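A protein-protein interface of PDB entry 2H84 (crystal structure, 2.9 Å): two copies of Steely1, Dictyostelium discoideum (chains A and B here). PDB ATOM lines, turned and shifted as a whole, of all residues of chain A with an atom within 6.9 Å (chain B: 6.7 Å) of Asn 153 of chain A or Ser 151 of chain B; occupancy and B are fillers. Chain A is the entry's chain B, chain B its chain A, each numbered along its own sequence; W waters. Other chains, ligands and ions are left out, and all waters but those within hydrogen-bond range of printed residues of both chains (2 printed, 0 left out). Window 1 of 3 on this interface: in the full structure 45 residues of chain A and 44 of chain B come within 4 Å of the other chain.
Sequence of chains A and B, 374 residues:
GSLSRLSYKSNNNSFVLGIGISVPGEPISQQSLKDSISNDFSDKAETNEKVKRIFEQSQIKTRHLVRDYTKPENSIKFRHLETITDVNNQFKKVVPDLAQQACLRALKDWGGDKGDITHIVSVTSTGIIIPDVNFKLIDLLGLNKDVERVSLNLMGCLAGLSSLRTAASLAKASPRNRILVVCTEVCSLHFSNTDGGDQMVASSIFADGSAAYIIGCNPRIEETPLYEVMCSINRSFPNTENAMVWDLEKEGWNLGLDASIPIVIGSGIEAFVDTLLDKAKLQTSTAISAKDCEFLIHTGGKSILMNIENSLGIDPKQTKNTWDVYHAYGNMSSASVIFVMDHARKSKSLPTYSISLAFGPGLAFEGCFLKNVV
Val 150 of chain A touches Leu 152 of chain B, and with the chains exchanged Leu 152 of chain A touches Val 150 of chain B.
Ser 151 of chain A touches Asn 153 of chain B, and with the chains exchanged Asn 153 of chain A touches Ser 151 of chain B.
Ser 151 of chain A touches Met 155 of chain B, and with the chains exchanged Met 155 of chain A touches Ser 151 of chain B.
Asn 153 of chain A touches Leu 154 of chain B, and with the chains exchanged Leu 154 of chain A touches Asn 153 of chain B.
Ser 151 of chain B touches just these residues of chain A: Ser 151 (3.2 Å), Leu 152 (3.5 Å), Asn 153 (3.3 Å) and Met 155 (3.5 Å).
Of the printed residues of chain B, Thr 166 of chain A touches Val 150 (3.9 Å).
Of the printed residues of chain B, Ser 151 of chain A touches Ser 151, Leu 152, Asn 153 and Met 155.
Of the printed residues of chain B, Met 155 of chain A touches Arg 149 (3.6 Å) and Ser 151 (3.5 Å).
Of the printed residues of chain B, Val 150 of chain A touches Leu 152 (3.8 Å) and Met 155 (3.97 Å).
Asp 132 of chain A touches none of the printed residues of chain B.
Ile 129 of chain A touches none of the printed residues of chain B.
The nearest residue of chain B that does not touch Asn 153 of chain A is Asp 132 of chain B (4.6 Å).
The nearest residue of chain A that does not touch Ser 151 of chain B is Leu 154 of chain A (4.6 Å).
The nearest printed residue of chain B that does not touch Leu 154 of chain A is Asp 132 of chain B (4.2 Å).
Water W2 bridges N of Asp 132 of chain A (2.7 Å) and O of Leu 154 of chain B (2.8 Å).
Water W1 bridges O of Met 155 of chain A (2.7 Å) and NH2 of Arg 149 of chain B (2.8 Å).
Val 150 of chain A touches Leu 152 of chain B (CG1 to CD2, 3.8 Å).
Val 150 of chain A touches Met 155 of chain B (N to CE, 3.97 Å).
O of Ser 151 of chain A touches CA of Leu 152 of chain B, 3.5 Å away.
CG of Met 155 of chain B touches OG of Ser 151 of chain A, at 3.5 Å.
Leu 152 of chain A touches Val 150 of chain B.
Leu 152 of chain A touches Ser 151 of chain B (CA to O, 3.5 Å).
Leu 154 of chain B touches Asn 153 of chain A.
Met 155 of chain A touches Arg 149 of chain B (CE to O, 3.6 Å).
Met 155 of chain A touches Ser 151 of chain B.
OG1 of Thr 166 of chain A touches CG2 of Val 150 of chain B (3.9 Å).
Of the 15 printed residues of chain B, 7 touch a printed residue of chain A.
Hydrophobic or aromatic side chains of chain B that line the printed part of chain A: Val 150, Leu 152, Leu 154 and Met 155.
Of the 19 printed residues of chain A, 8 touch a printed residue of chain B.
Printed residues of chain A that touch a printed residue of chain B: Ile 128, Val 150, Ser 151, Leu 152, Asn 153, Leu 154, Met 155 and Thr 166.
Hydrophobic or aromatic side chains of chain A within 4 Å of the printed part of chain B: Ile 128, Val 150, Leu 152, Leu 154 and Met 155.
N of Asn 153 of chain A sits at hydrogen-bond distance from O of Ser 151 of chain B (3.3 Å).
The backbone NH (N) of Asn 153 of chain B lies within hydrogen-bond range of the backbone carbonyl oxygen (O) of Ser 151 of chain A (3.3 Å).
The backbone carbonyl oxygen (O) of Asn 153 of chain A sits at hydrogen-bond distance from the side-chain amide nitrogen (ND2) of Asn 153 of chain B, 2.7 Å away.
The backbone carbonyl oxygen of Ser 151 of chain A sits close to the backbone carbonyl oxygen of Ser 151 of chain B (3.2 Å).
The backbone NH (N) of Val 150 of chain B is in hydrogen-bond range of the backbone carbonyl oxygen (O) of Ile 120 of chain B, at 3.1 Å.
The backbone NH (N) of Ser 122 of chain B lies within hydrogen-bond range of the backbone carbonyl oxygen (O) of Val 150 of chain B, at 3.0 Å.
ND2 of Asn 134 of chain B sits close to NE of Arg 149 of chain B (2.9 Å).
O of Ser 122 of chain A lies within hydrogen-bond range of N of Leu 152 of chain A (2.9 Å).
The backbone NH (N) of Thr 124 of chain A sits at hydrogen-bond distance from the side-chain amide oxygen (OD1) of Asn 153 of chain A (3.3 Å).
The backbone NH (N) of Leu 154 of chain A lies within hydrogen-bond range of the backbone carbonyl oxygen (O) of Thr 124 of chain A, 3.3 Å away.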
ATOM      1  N   SER A 122     -25.857 -21.229 -30.098  1.00  0.00           N
ATOM      2  CA  SER A 122     -25.263 -21.490 -31.410  1.00  0.00           C
ATOM      3  C   SER A 122     -23.883 -22.132 -31.210  1.00  0.00           C
ATOM      4  O   SER A 122     -23.144 -21.771 -30.280  1.00  0.00           O
ATOM      5  CB  SER A 122     -25.150 -20.154 -32.167  1.00  0.00           C
ATOM      6  OG  SER A 122     -24.254 -20.206 -33.264  1.00  0.00           O
ATOM      7  N   VAL A 123     -23.545 -23.086 -32.076  1.00  0.00           N
ATOM      8  CA  VAL A 123     -22.263 -23.792 -31.995  1.00  0.00           C
ATOM      9  C   VAL A 123     -21.617 -24.133 -33.338  1.00  0.00           C
ATOM     10  O   VAL A 123     -22.249 -24.740 -34.211  1.00  0.00           O
ATOM     11  CB  VAL A 123     -22.399 -25.129 -31.221  1.00  0.00           C
ATOM     12  CG1 VAL A 123     -21.072 -25.849 -31.200  1.00  0.00           C
ATOM     13  CG2 VAL A 123     -22.854 -24.886 -29.803  1.00  0.00           C
ATOM     14  N   THR A 124     -20.351 -23.750 -33.496  1.00  0.00           N
ATOM     15  CA  THR A 124     -19.608 -24.061 -34.722  1.00  0.00           C
ATOM     16  C   THR A 124     -18.175 -23.579 -34.641  1.00  0.00           C
ATOM     17  O   THR A 124     -17.874 -22.658 -33.886  1.00  0.00           O
ATOM     18  CB  THR A 124     -20.249 -23.439 -35.994  1.00  0.00           C
ATOM     19  OG1 THR A 124     -19.760 -24.127 -37.138  1.00  0.00           O
ATOM     20  CG2 THR A 124     -19.824 -22.035 -36.222  1.00  0.00           C
ATOM     21  N   SER A 125     -17.306 -24.217 -35.429  1.00  0.00           N
ATOM     22  CA  SER A 125     -15.891 -23.883 -35.496  1.00  0.00           C
ATOM     23  C   SER A 125     -15.376 -23.946 -36.929  1.00  0.00           C
ATOM     24  O   SER A 125     -14.177 -23.831 -37.154  1.00  0.00           O
ATOM     25  CB  SER A 125     -15.065 -24.834 -34.629  1.00  0.00           C
ATOM     26  OG  SER A 125     -15.530 -24.860 -33.292  1.00  0.00           O
ATOM     27  N   GLY A 127     -16.510 -21.846 -39.437  1.00  0.00           N
ATOM     28  CA  GLY A 127     -16.734 -20.583 -40.112  1.00  0.00           C
ATOM     29  C   GLY A 127     -17.071 -19.491 -39.118  1.00  0.00           C
ATOM     30  O   GLY A 127     -17.606 -19.757 -38.045  1.00  0.00           O
ATOM     31  N   ILE A 128     -16.756 -18.251 -39.468  1.00  0.00           N
ATOM     32  CA  ILE A 128     -17.039 -17.133 -38.589  1.00  0.00           C
ATOM     33  C   ILE A 128     -18.171 -16.267 -39.108  1.00  0.00           C
ATOM     34  O   ILE A 128     -18.080 -15.693 -40.193  1.00  0.00           O
ATOM     35  CB  ILE A 128     -15.811 -16.245 -38.413  1.00  0.00           C
ATOM     36  CG1 ILE A 128     -14.640 -17.078 -37.881  1.00  0.00           C
ATOM     37  CG2 ILE A 128     -16.138 -15.114 -37.458  1.00  0.00           C
ATOM     38  CD1 ILE A 128     -14.949 -17.800 -36.570  1.00  0.00           C
ATOM     39  N   ILE A 129     -19.251 -16.193 -38.334  1.00  0.00           N
ATOM     40  CA  ILE A 129     -20.399 -15.370 -38.708  1.00  0.00           C
ATOM     41  C   ILE A 129     -20.736 -14.393 -37.605  1.00  0.00           C
ATOM     42  O   ILE A 129     -20.967 -14.802 -36.473  1.00  0.00           O
ATOM     43  CB  ILE A 129     -21.638 -16.200 -38.989  1.00  0.00           C
ATOM     44  CG1 ILE A 129     -21.310 -17.271 -40.023  1.00  0.00           C
ATOM     45  CG2 ILE A 129     -22.710 -15.315 -39.563  1.00  0.00           C
ATOM     46  CD1 ILE A 129     -22.502 -18.109 -40.472  1.00  0.00           C
ATOM     47  N   ASP A 132     -23.562 -13.702 -34.793  1.00  0.00           N
ATOM     48  CA  ASP A 132     -23.554 -15.164 -34.780  1.00  0.00           C
ATOM     49  C   ASP A 132     -24.883 -15.833 -35.167  1.00  0.00           C
ATOM     50  O   ASP A 132     -25.937 -15.208 -35.172  1.00  0.00           O
ATOM     51  CB  ASP A 132     -23.127 -15.650 -33.405  1.00  0.00           C
ATOM     52  CG  ASP A 132     -22.585 -17.050 -33.432  1.00  0.00           C
ATOM     53  OD1 ASP A 132     -22.411 -17.633 -32.346  1.00  0.00           O
ATOM     54  OD2 ASP A 132     -22.320 -17.573 -34.530  1.00  0.00           O
ATOM     55  N   VAL A 133     -24.816 -17.120 -35.474  1.00  0.00           N
ATOM     56  CA  VAL A 133     -25.986 -17.879 -35.880  1.00  0.00           C
ATOM     57  C   VAL A 133     -27.176 -17.784 -34.923  1.00  0.00           C
ATOM     58  O   VAL A 133     -28.318 -17.699 -35.367  1.00  0.00           O
ATOM     59  CB  VAL A 133     -25.641 -19.374 -36.069  1.00  0.00           C
ATOM     60  CG1 VAL A 133     -26.732 -20.074 -36.867  1.00  0.00           C
ATOM     61  CG2 VAL A 133     -24.316 -19.510 -36.771  1.00  0.00           C
ATOM     62  N   ASN A 134     -26.923 -17.798 -33.616  1.00  0.00           N
ATOM     63  CA  ASN A 134     -28.021 -17.732 -32.661  1.00  0.00           C
ATOM     64  C   ASN A 134     -28.829 -16.436 -32.751  1.00  0.00           C
ATOM     65  O   ASN A 134     -30.034 -16.427 -32.476  1.00  0.00           O
ATOM     66  CB  ASN A 134     -27.519 -17.963 -31.225  1.00  0.00           C
ATOM     67  CG  ASN A 134     -26.451 -16.992 -30.809  1.00  0.00           C
ATOM     68  OD1 ASN A 134     -26.701 -16.019 -30.155  1.00  0.00           O
ATOM     69  ND2 ASN A 134     -25.258 -17.259 -31.199  1.00  0.00           N
ATOM     70  N   VAL A 150     -26.175 -17.322 -26.509  1.00  0.00           N
ATOM     71  CA  VAL A 150     -24.930 -17.958 -26.086  1.00  0.00           C
ATOM     72  C   VAL A 150     -24.221 -18.474 -27.331  1.00  0.00           C
ATOM     73  O   VAL A 150     -24.751 -19.343 -28.022  1.00  0.00           O
ATOM     74  CB  VAL A 150     -25.206 -19.184 -25.163  1.00  0.00           C
ATOM     75  CG1 VAL A 150     -23.903 -19.843 -24.774  1.00  0.00           C
ATOM     76  CG2 VAL A 150     -25.965 -18.758 -23.923  1.00  0.00           C
ATOM     77  N   SER A 151     -23.037 -17.941 -27.624  1.00  0.00           N
ATOM     78  CA  SER A 151     -22.255 -18.398 -28.783  1.00  0.00           C
ATOM     79  C   SER A 151     -21.084 -19.324 -28.382  1.00  0.00           C
ATOM     80  O   SER A 151     -20.008 -18.837 -28.036  1.00  0.00           O
ATOM     81  CB  SER A 151     -21.694 -17.199 -29.555  1.00  0.00           C
ATOM     82  OG  SER A 151     -22.728 -16.387 -30.076  1.00  0.00           O
ATOM     83  N   LEU A 152     -21.290 -20.647 -28.414  1.00  0.00           N
ATOM     84  CA  LEU A 152     -20.213 -21.606 -28.077  1.00  0.00           C
ATOM     85  C   LEU A 152     -19.386 -21.933 -29.317  1.00  0.00           C
ATOM     86  O   LEU A 152     -19.576 -22.987 -29.930  1.00  0.00           O
ATOM     87  CB  LEU A 152     -20.766 -22.936 -27.542  1.00  0.00           C
ATOM     88  CG  LEU A 152     -20.825 -23.305 -26.052  1.00  0.00           C
ATOM     89  CD1 LEU A 152     -20.817 -24.834 -25.975  1.00  0.00           C
ATOM     90  CD2 LEU A 152     -19.644 -22.724 -25.249  1.00  0.00           C
ATOM     91  N   ASN A 153     -18.452 -21.058 -29.672  1.00  0.00           N
ATOM     92  CA  ASN A 153     -17.660 -21.282 -30.870  1.00  0.00           C
ATOM     93  C   ASN A 153     -16.169 -21.492 -30.633  1.00  0.00           C
ATOM     94  O   ASN A 153     -15.597 -21.007 -29.648  1.00  0.00           O
ATOM     95  CB  ASN A 153     -17.872 -20.115 -31.840  1.00  0.00           C
ATOM     96  CG  ASN A 153     -19.338 -19.773 -32.021  1.00  0.00           C
ATOM     97  OD1 ASN A 153     -20.133 -20.609 -32.441  1.00  0.00           O
ATOM     98  ND2 ASN A 153     -19.703 -18.537 -31.699  1.00  0.00           N
ATOM     99  N   LEU A 154     -15.556 -22.229 -31.558  1.00  0.00           N
ATOM    100  CA  LEU A 154     -14.130 -22.530 -31.527  1.00  0.00           C
ATOM    101  C   LEU A 154     -13.763 -23.661 -30.563  1.00  0.00           C
ATOM    102  O   LEU A 154     -12.629 -23.722 -30.072  1.00  0.00           O
ATOM    103  CB  LEU A 154     -13.329 -21.263 -31.183  1.00  0.00           C
ATOM    104  CG  LEU A 154     -13.602 -20.046 -32.071  1.00  0.00           C
ATOM    105  CD1 LEU A 154     -12.618 -18.944 -31.738  1.00  0.00           C
ATOM    106  CD2 LEU A 154     -13.473 -20.428 -33.522  1.00  0.00           C
ATOM    107  N   MET A 155     -14.705 -24.559 -30.288  1.00  0.00           N
ATOM    108  CA  MET A 155     -14.391 -25.663 -29.387  1.00  0.00           C
ATOM    109  C   MET A 155     -14.037 -26.932 -30.143  1.00  0.00           C
ATOM    110  O   MET A 155     -13.561 -27.911 -29.562  1.00  0.00           O
ATOM    111  CB  MET A 155     -15.535 -25.931 -28.410  1.00  0.00           C
ATOM    112  CG  MET A 155     -15.724 -24.808 -27.411  1.00  0.00           C
ATOM    113  SD  MET A 155     -16.726 -25.245 -25.981  1.00  0.00           S
ATOM    114  CE  MET A 155     -15.476 -25.556 -24.797  1.00  0.00           C
ATOM    115  N   GLY A 156     -14.263 -26.911 -31.449  1.00  0.00           N
ATOM    116  CA  GLY A 156     -13.927 -28.066 -32.256  1.00  0.00           C
ATOM    117  C   GLY A 156     -14.912 -29.213 -32.242  1.00  0.00           C
ATOM    118  O   GLY A 156     -16.070 -29.062 -31.829  1.00  0.00           O
ATOM    119  N   ALA A 159     -17.383 -29.883 -29.416  1.00  0.00           N
ATOM    120  CA  ALA A 159     -18.412 -28.879 -29.125  1.00  0.00           C
ATOM    121  C   ALA A 159     -19.778 -29.504 -28.875  1.00  0.00           C
ATOM    122  O   ALA A 159     -20.616 -28.969 -28.145  1.00  0.00           O
ATOM    123  CB  ALA A 159     -18.507 -27.888 -30.244  1.00  0.00           C
ATOM    124  N   THR A 166     -22.866 -27.520 -20.989  1.00  0.00           N
ATOM    125  CA  THR A 166     -23.203 -26.166 -20.595  1.00  0.00           C
ATOM    126  C   THR A 166     -24.719 -25.928 -20.534  1.00  0.00           C
ATOM    127  O   THR A 166     -25.207 -25.302 -19.592  1.00  0.00           O
ATOM    128  CB  THR A 166     -22.570 -25.153 -21.534  1.00  0.00           C
ATOM    129  OG1 THR A 166     -21.156 -25.363 -21.559  1.00  0.00           O
ATOM    130  CG2 THR A 166     -22.849 -23.748 -21.048  1.00  0.00           C
ATOM    131  N   ILE B 120     -14.123 -22.562 -16.232  1.00  0.00           N
ATOM    132  CA  ILE B 120     -13.223 -21.597 -16.835  1.00  0.00           C
ATOM    133  C   ILE B 120     -13.887 -21.159 -18.151  1.00  0.00           C
ATOM    134  O   ILE B 120     -14.161 -21.974 -19.033  1.00  0.00           O
ATOM    135  CB  ILE B 120     -11.816 -22.236 -17.025  1.00  0.00           C
ATOM    136  CG1 ILE B 120     -10.720 -21.175 -16.912  1.00  0.00           C
ATOM    137  CG2 ILE B 120     -11.752 -23.047 -18.279  1.00  0.00           C
ATOM    138  CD1 ILE B 120     -10.612 -20.186 -17.952  1.00  0.00           C
ATOM    139  N   VAL B 121     -14.198 -19.868 -18.240  1.00  0.00           N
ATOM    140  CA  VAL B 121     -14.846 -19.298 -19.410  1.00  0.00           C
ATOM    141  C   VAL B 121     -13.975 -18.273 -20.119  1.00  0.00           C
ATOM    142  O   VAL B 121     -13.623 -17.239 -19.555  1.00  0.00           O
ATOM    143  CB  VAL B 121     -16.151 -18.602 -19.034  1.00  0.00           C
ATOM    144  CG1 VAL B 121     -16.866 -18.116 -20.309  1.00  0.00           C
ATOM    145  CG2 VAL B 121     -17.026 -19.539 -18.239  1.00  0.00           C
ATOM    146  N   SER B 122     -13.667 -18.566 -21.375  1.00  0.00           N
ATOM    147  CA  SER B 122     -12.837 -17.728 -22.226  1.00  0.00           C
ATOM    148  C   SER B 122     -13.757 -16.939 -23.163  1.00  0.00           C
ATOM    149  O   SER B 122     -14.744 -17.490 -23.655  1.00  0.00           O
ATOM    150  CB  SER B 122     -11.891 -18.641 -23.014  1.00  0.00           C
ATOM    151  OG  SER B 122     -11.265 -17.981 -24.097  1.00  0.00           O
ATOM    152  N   VAL B 123     -13.437 -15.661 -23.394  1.00  0.00           N
ATOM    153  CA  VAL B 123     -14.233 -14.770 -24.254  1.00  0.00           C
ATOM    154  C   VAL B 123     -13.381 -13.832 -25.138  1.00  0.00           C
ATOM    155  O   VAL B 123     -12.466 -13.164 -24.656  1.00  0.00           O
ATOM    156  CB  VAL B 123     -15.178 -13.886 -23.391  1.00  0.00           C
ATOM    157  CG1 VAL B 123     -15.936 -12.915 -24.269  1.00  0.00           C
ATOM    158  CG2 VAL B 123     -16.148 -14.753 -22.619  1.00  0.00           C
ATOM    159  N   ASP B 132      -8.829 -23.144 -27.662  1.00  0.00           N
ATOM    160  CA  ASP B 132      -9.187 -21.819 -27.164  1.00  0.00           C
ATOM    161  C   ASP B 132      -8.420 -21.392 -25.917  1.00  0.00           C
ATOM    162  O   ASP B 132      -7.794 -22.210 -25.257  1.00  0.00           O
ATOM    163  CB  ASP B 132     -10.676 -21.772 -26.871  1.00  0.00           C
ATOM    164  CG  ASP B 132     -11.214 -20.364 -26.843  1.00  0.00           C
ATOM    165  OD1 ASP B 132     -12.380 -20.198 -26.451  1.00  0.00           O
ATOM    166  OD2 ASP B 132     -10.484 -19.424 -27.215  1.00  0.00           O
ATOM    167  N   VAL B 133      -8.489 -20.105 -25.594  1.00  0.00           N
ATOM    168  CA  VAL B 133      -7.797 -19.560 -24.431  1.00  0.00           C
ATOM    169  C   VAL B 133      -8.100 -20.275 -23.113  1.00  0.00           C
ATOM    170  O   VAL B 133      -7.199 -20.492 -22.307  1.00  0.00           O
ATOM    171  CB  VAL B 133      -8.121 -18.073 -24.254  1.00  0.00           C
ATOM    172  CG1 VAL B 133      -7.281 -17.479 -23.147  1.00  0.00           C
ATOM    173  CG2 VAL B 133      -7.864 -17.340 -25.551  1.00  0.00           C
ATOM    174  N   ASN B 134      -9.355 -20.644 -22.877  1.00  0.00           N
ATOM    175  CA  ASN B 134      -9.679 -21.312 -21.624  1.00  0.00           C
ATOM    176  C   ASN B 134      -8.927 -22.621 -21.424  1.00  0.00           C
ATOM    177  O   ASN B 134      -8.625 -22.981 -20.288  1.00  0.00           O
ATOM    178  CB  ASN B 134     -11.189 -21.559 -21.492  1.00  0.00           C
ATOM    179  CG  ASN B 134     -11.774 -22.302 -22.672  1.00  0.00           C
ATOM    180  OD1 ASN B 134     -12.267 -21.720 -23.595  1.00  0.00           O
ATOM    181  ND2 ASN B 134     -11.718 -23.585 -22.633  1.00  0.00           N
ATOM    182  N   PHE B 135      -8.630 -23.339 -22.510  1.00  0.00           N
ATOM    183  CA  PHE B 135      -7.899 -24.607 -22.402  1.00  0.00           C
ATOM    184  C   PHE B 135      -6.435 -24.342 -22.068  1.00  0.00           C
ATOM    185  O   PHE B 135      -5.858 -24.969 -21.171  1.00  0.00           O
ATOM    186  CB  PHE B 135      -7.966 -25.391 -23.711  1.00  0.00           C
ATOM    187  CG  PHE B 135      -7.158 -26.670 -23.695  1.00  0.00           C
ATOM    188  CD1 PHE B 135      -7.741 -27.875 -23.298  1.00  0.00           C
ATOM    189  CD2 PHE B 135      -5.815 -26.667 -24.058  1.00  0.00           C
ATOM    190  CE1 PHE B 135      -7.005 -29.042 -23.249  1.00  0.00           C
ATOM    191  CE2 PHE B 135      -5.077 -27.834 -24.010  1.00  0.00           C
ATOM    192  CZ  PHE B 135      -5.678 -29.023 -23.609  1.00  0.00           C
ATOM    193  N   ARG B 149     -14.849 -26.374 -19.325  1.00  0.00           N
ATOM    194  CA  ARG B 149     -14.552 -25.307 -20.282  1.00  0.00           C
ATOM    195  C   ARG B 149     -15.768 -24.763 -21.038  1.00  0.00           C
ATOM    196  O   ARG B 149     -16.685 -25.505 -21.392  1.00  0.00           O
ATOM    197  CB  ARG B 149     -13.524 -25.764 -21.320  1.00  0.00           C
ATOM    198  CG  ARG B 149     -12.555 -26.833 -20.867  1.00  0.00           C
ATOM    199  CD  ARG B 149     -11.253 -26.787 -21.673  1.00  0.00           C
ATOM    200  NE  ARG B 149     -11.417 -26.469 -23.096  1.00  0.00           N
ATOM    201  CZ  ARG B 149     -12.011 -27.254 -23.993  1.00  0.00           C
ATOM    202  NH1 ARG B 149     -12.522 -28.430 -23.635  1.00  0.00           N
ATOM    203  NH2 ARG B 149     -12.076 -26.867 -25.260  1.00  0.00           N
ATOM    204  N   VAL B 150     -15.744 -23.456 -21.288  1.00  0.00           N
ATOM    205  CA  VAL B 150     -16.799 -22.750 -22.010  1.00  0.00           C
ATOM    206  C   VAL B 150     -16.157 -21.682 -22.895  1.00  0.00           C
ATOM    207  O   VAL B 150     -15.506 -20.778 -22.381  1.00  0.00           O
ATOM    208  CB  VAL B 150     -17.768 -22.048 -21.039  1.00  0.00           C
ATOM    209  CG1 VAL B 150     -18.858 -21.344 -21.814  1.00  0.00           C
ATOM    210  CG2 VAL B 150     -18.369 -23.052 -20.097  1.00  0.00           C
ATOM    211  N   SER B 151     -16.324 -21.782 -24.214  1.00  0.00           N
ATOM    212  CA  SER B 151     -15.752 -20.781 -25.130  1.00  0.00           C
ATOM    213  C   SER B 151     -16.800 -19.808 -25.687  1.00  0.00           C
ATOM    214  O   SER B 151     -17.400 -20.081 -26.716  1.00  0.00           O
ATOM    215  CB  SER B 151     -15.057 -21.463 -26.313  1.00  0.00           C
ATOM    216  OG  SER B 151     -13.884 -22.162 -25.925  1.00  0.00           O
ATOM    217  N   LEU B 152     -17.027 -18.685 -25.011  1.00  0.00           N
ATOM    218  CA  LEU B 152     -17.988 -17.684 -25.484  1.00  0.00           C
ATOM    219  C   LEU B 152     -17.292 -16.753 -26.479  1.00  0.00           C
ATOM    220  O   LEU B 152     -16.829 -15.672 -26.099  1.00  0.00           O
ATOM    221  CB  LEU B 152     -18.513 -16.812 -24.336  1.00  0.00           C
ATOM    222  CG  LEU B 152     -19.860 -17.049 -23.651  1.00  0.00           C
ATOM    223  CD1 LEU B 152     -20.303 -15.725 -23.010  1.00  0.00           C
ATOM    224  CD2 LEU B 152     -20.909 -17.528 -24.653  1.00  0.00           C
ATOM    225  N   ASN B 153     -17.218 -17.152 -27.745  1.00  0.00           N
ATOM    226  CA  ASN B 153     -16.558 -16.320 -28.735  1.00  0.00           C
ATOM    227  C   ASN B 153     -17.476 -15.854 -29.872  1.00  0.00           C
ATOM    228  O   ASN B 153     -18.487 -16.486 -30.187  1.00  0.00           O
ATOM    229  CB  ASN B 153     -15.375 -17.085 -29.314  1.00  0.00           C
ATOM    230  CG  ASN B 153     -14.524 -17.728 -28.244  1.00  0.00           C
ATOM    231  OD1 ASN B 153     -13.979 -17.044 -27.372  1.00  0.00           O
ATOM    232  ND2 ASN B 153     -14.403 -19.054 -28.301  1.00  0.00           N
ATOM    233  N   LEU B 154     -17.104 -14.736 -30.485  1.00  0.00           N
ATOM    234  CA  LEU B 154     -17.848 -14.176 -31.607  1.00  0.00           C
ATOM    235  C   LEU B 154     -19.112 -13.441 -31.210  1.00  0.00           C
ATOM    236  O   LEU B 154     -20.037 -13.344 -32.001  1.00  0.00           O
ATOM    237  CB  LEU B 154     -18.192 -15.275 -32.623  1.00  0.00           C
ATOM    238  CG  LEU B 154     -17.008 -16.107 -33.149  1.00  0.00           C
ATOM    239  CD1 LEU B 154     -17.460 -16.995 -34.292  1.00  0.00           C
ATOM    240  CD2 LEU B 154     -15.898 -15.192 -33.621  1.00  0.00           C
ATOM    241  N   MET B 155     -19.158 -12.911 -29.993  1.00  0.00           N
ATOM    242  CA  MET B 155     -20.343 -12.179 -29.560  1.00  0.00           C
ATOM    243  C   MET B 155     -20.127 -10.675 -29.654  1.00  0.00           C
ATOM    244  O   MET B 155     -21.068  -9.890 -29.502  1.00  0.00           O
ATOM    245  CB  MET B 155     -20.741 -12.579 -28.137  1.00  0.00           C
ATOM    246  CG  MET B 155     -21.225 -14.015 -28.051  1.00  0.00           C
ATOM    247  SD  MET B 155     -22.107 -14.412 -26.556  1.00  0.00           S
ATOM    248  CE  MET B 155     -23.769 -14.219 -27.084  1.00  0.00           C
HETATM  249  O   HOH W   1     -11.418 -27.552 -27.914  1.00  0.00           O
HETATM  250  O   HOH W   2     -22.718 -12.577 -32.515  1.00  0.00           O
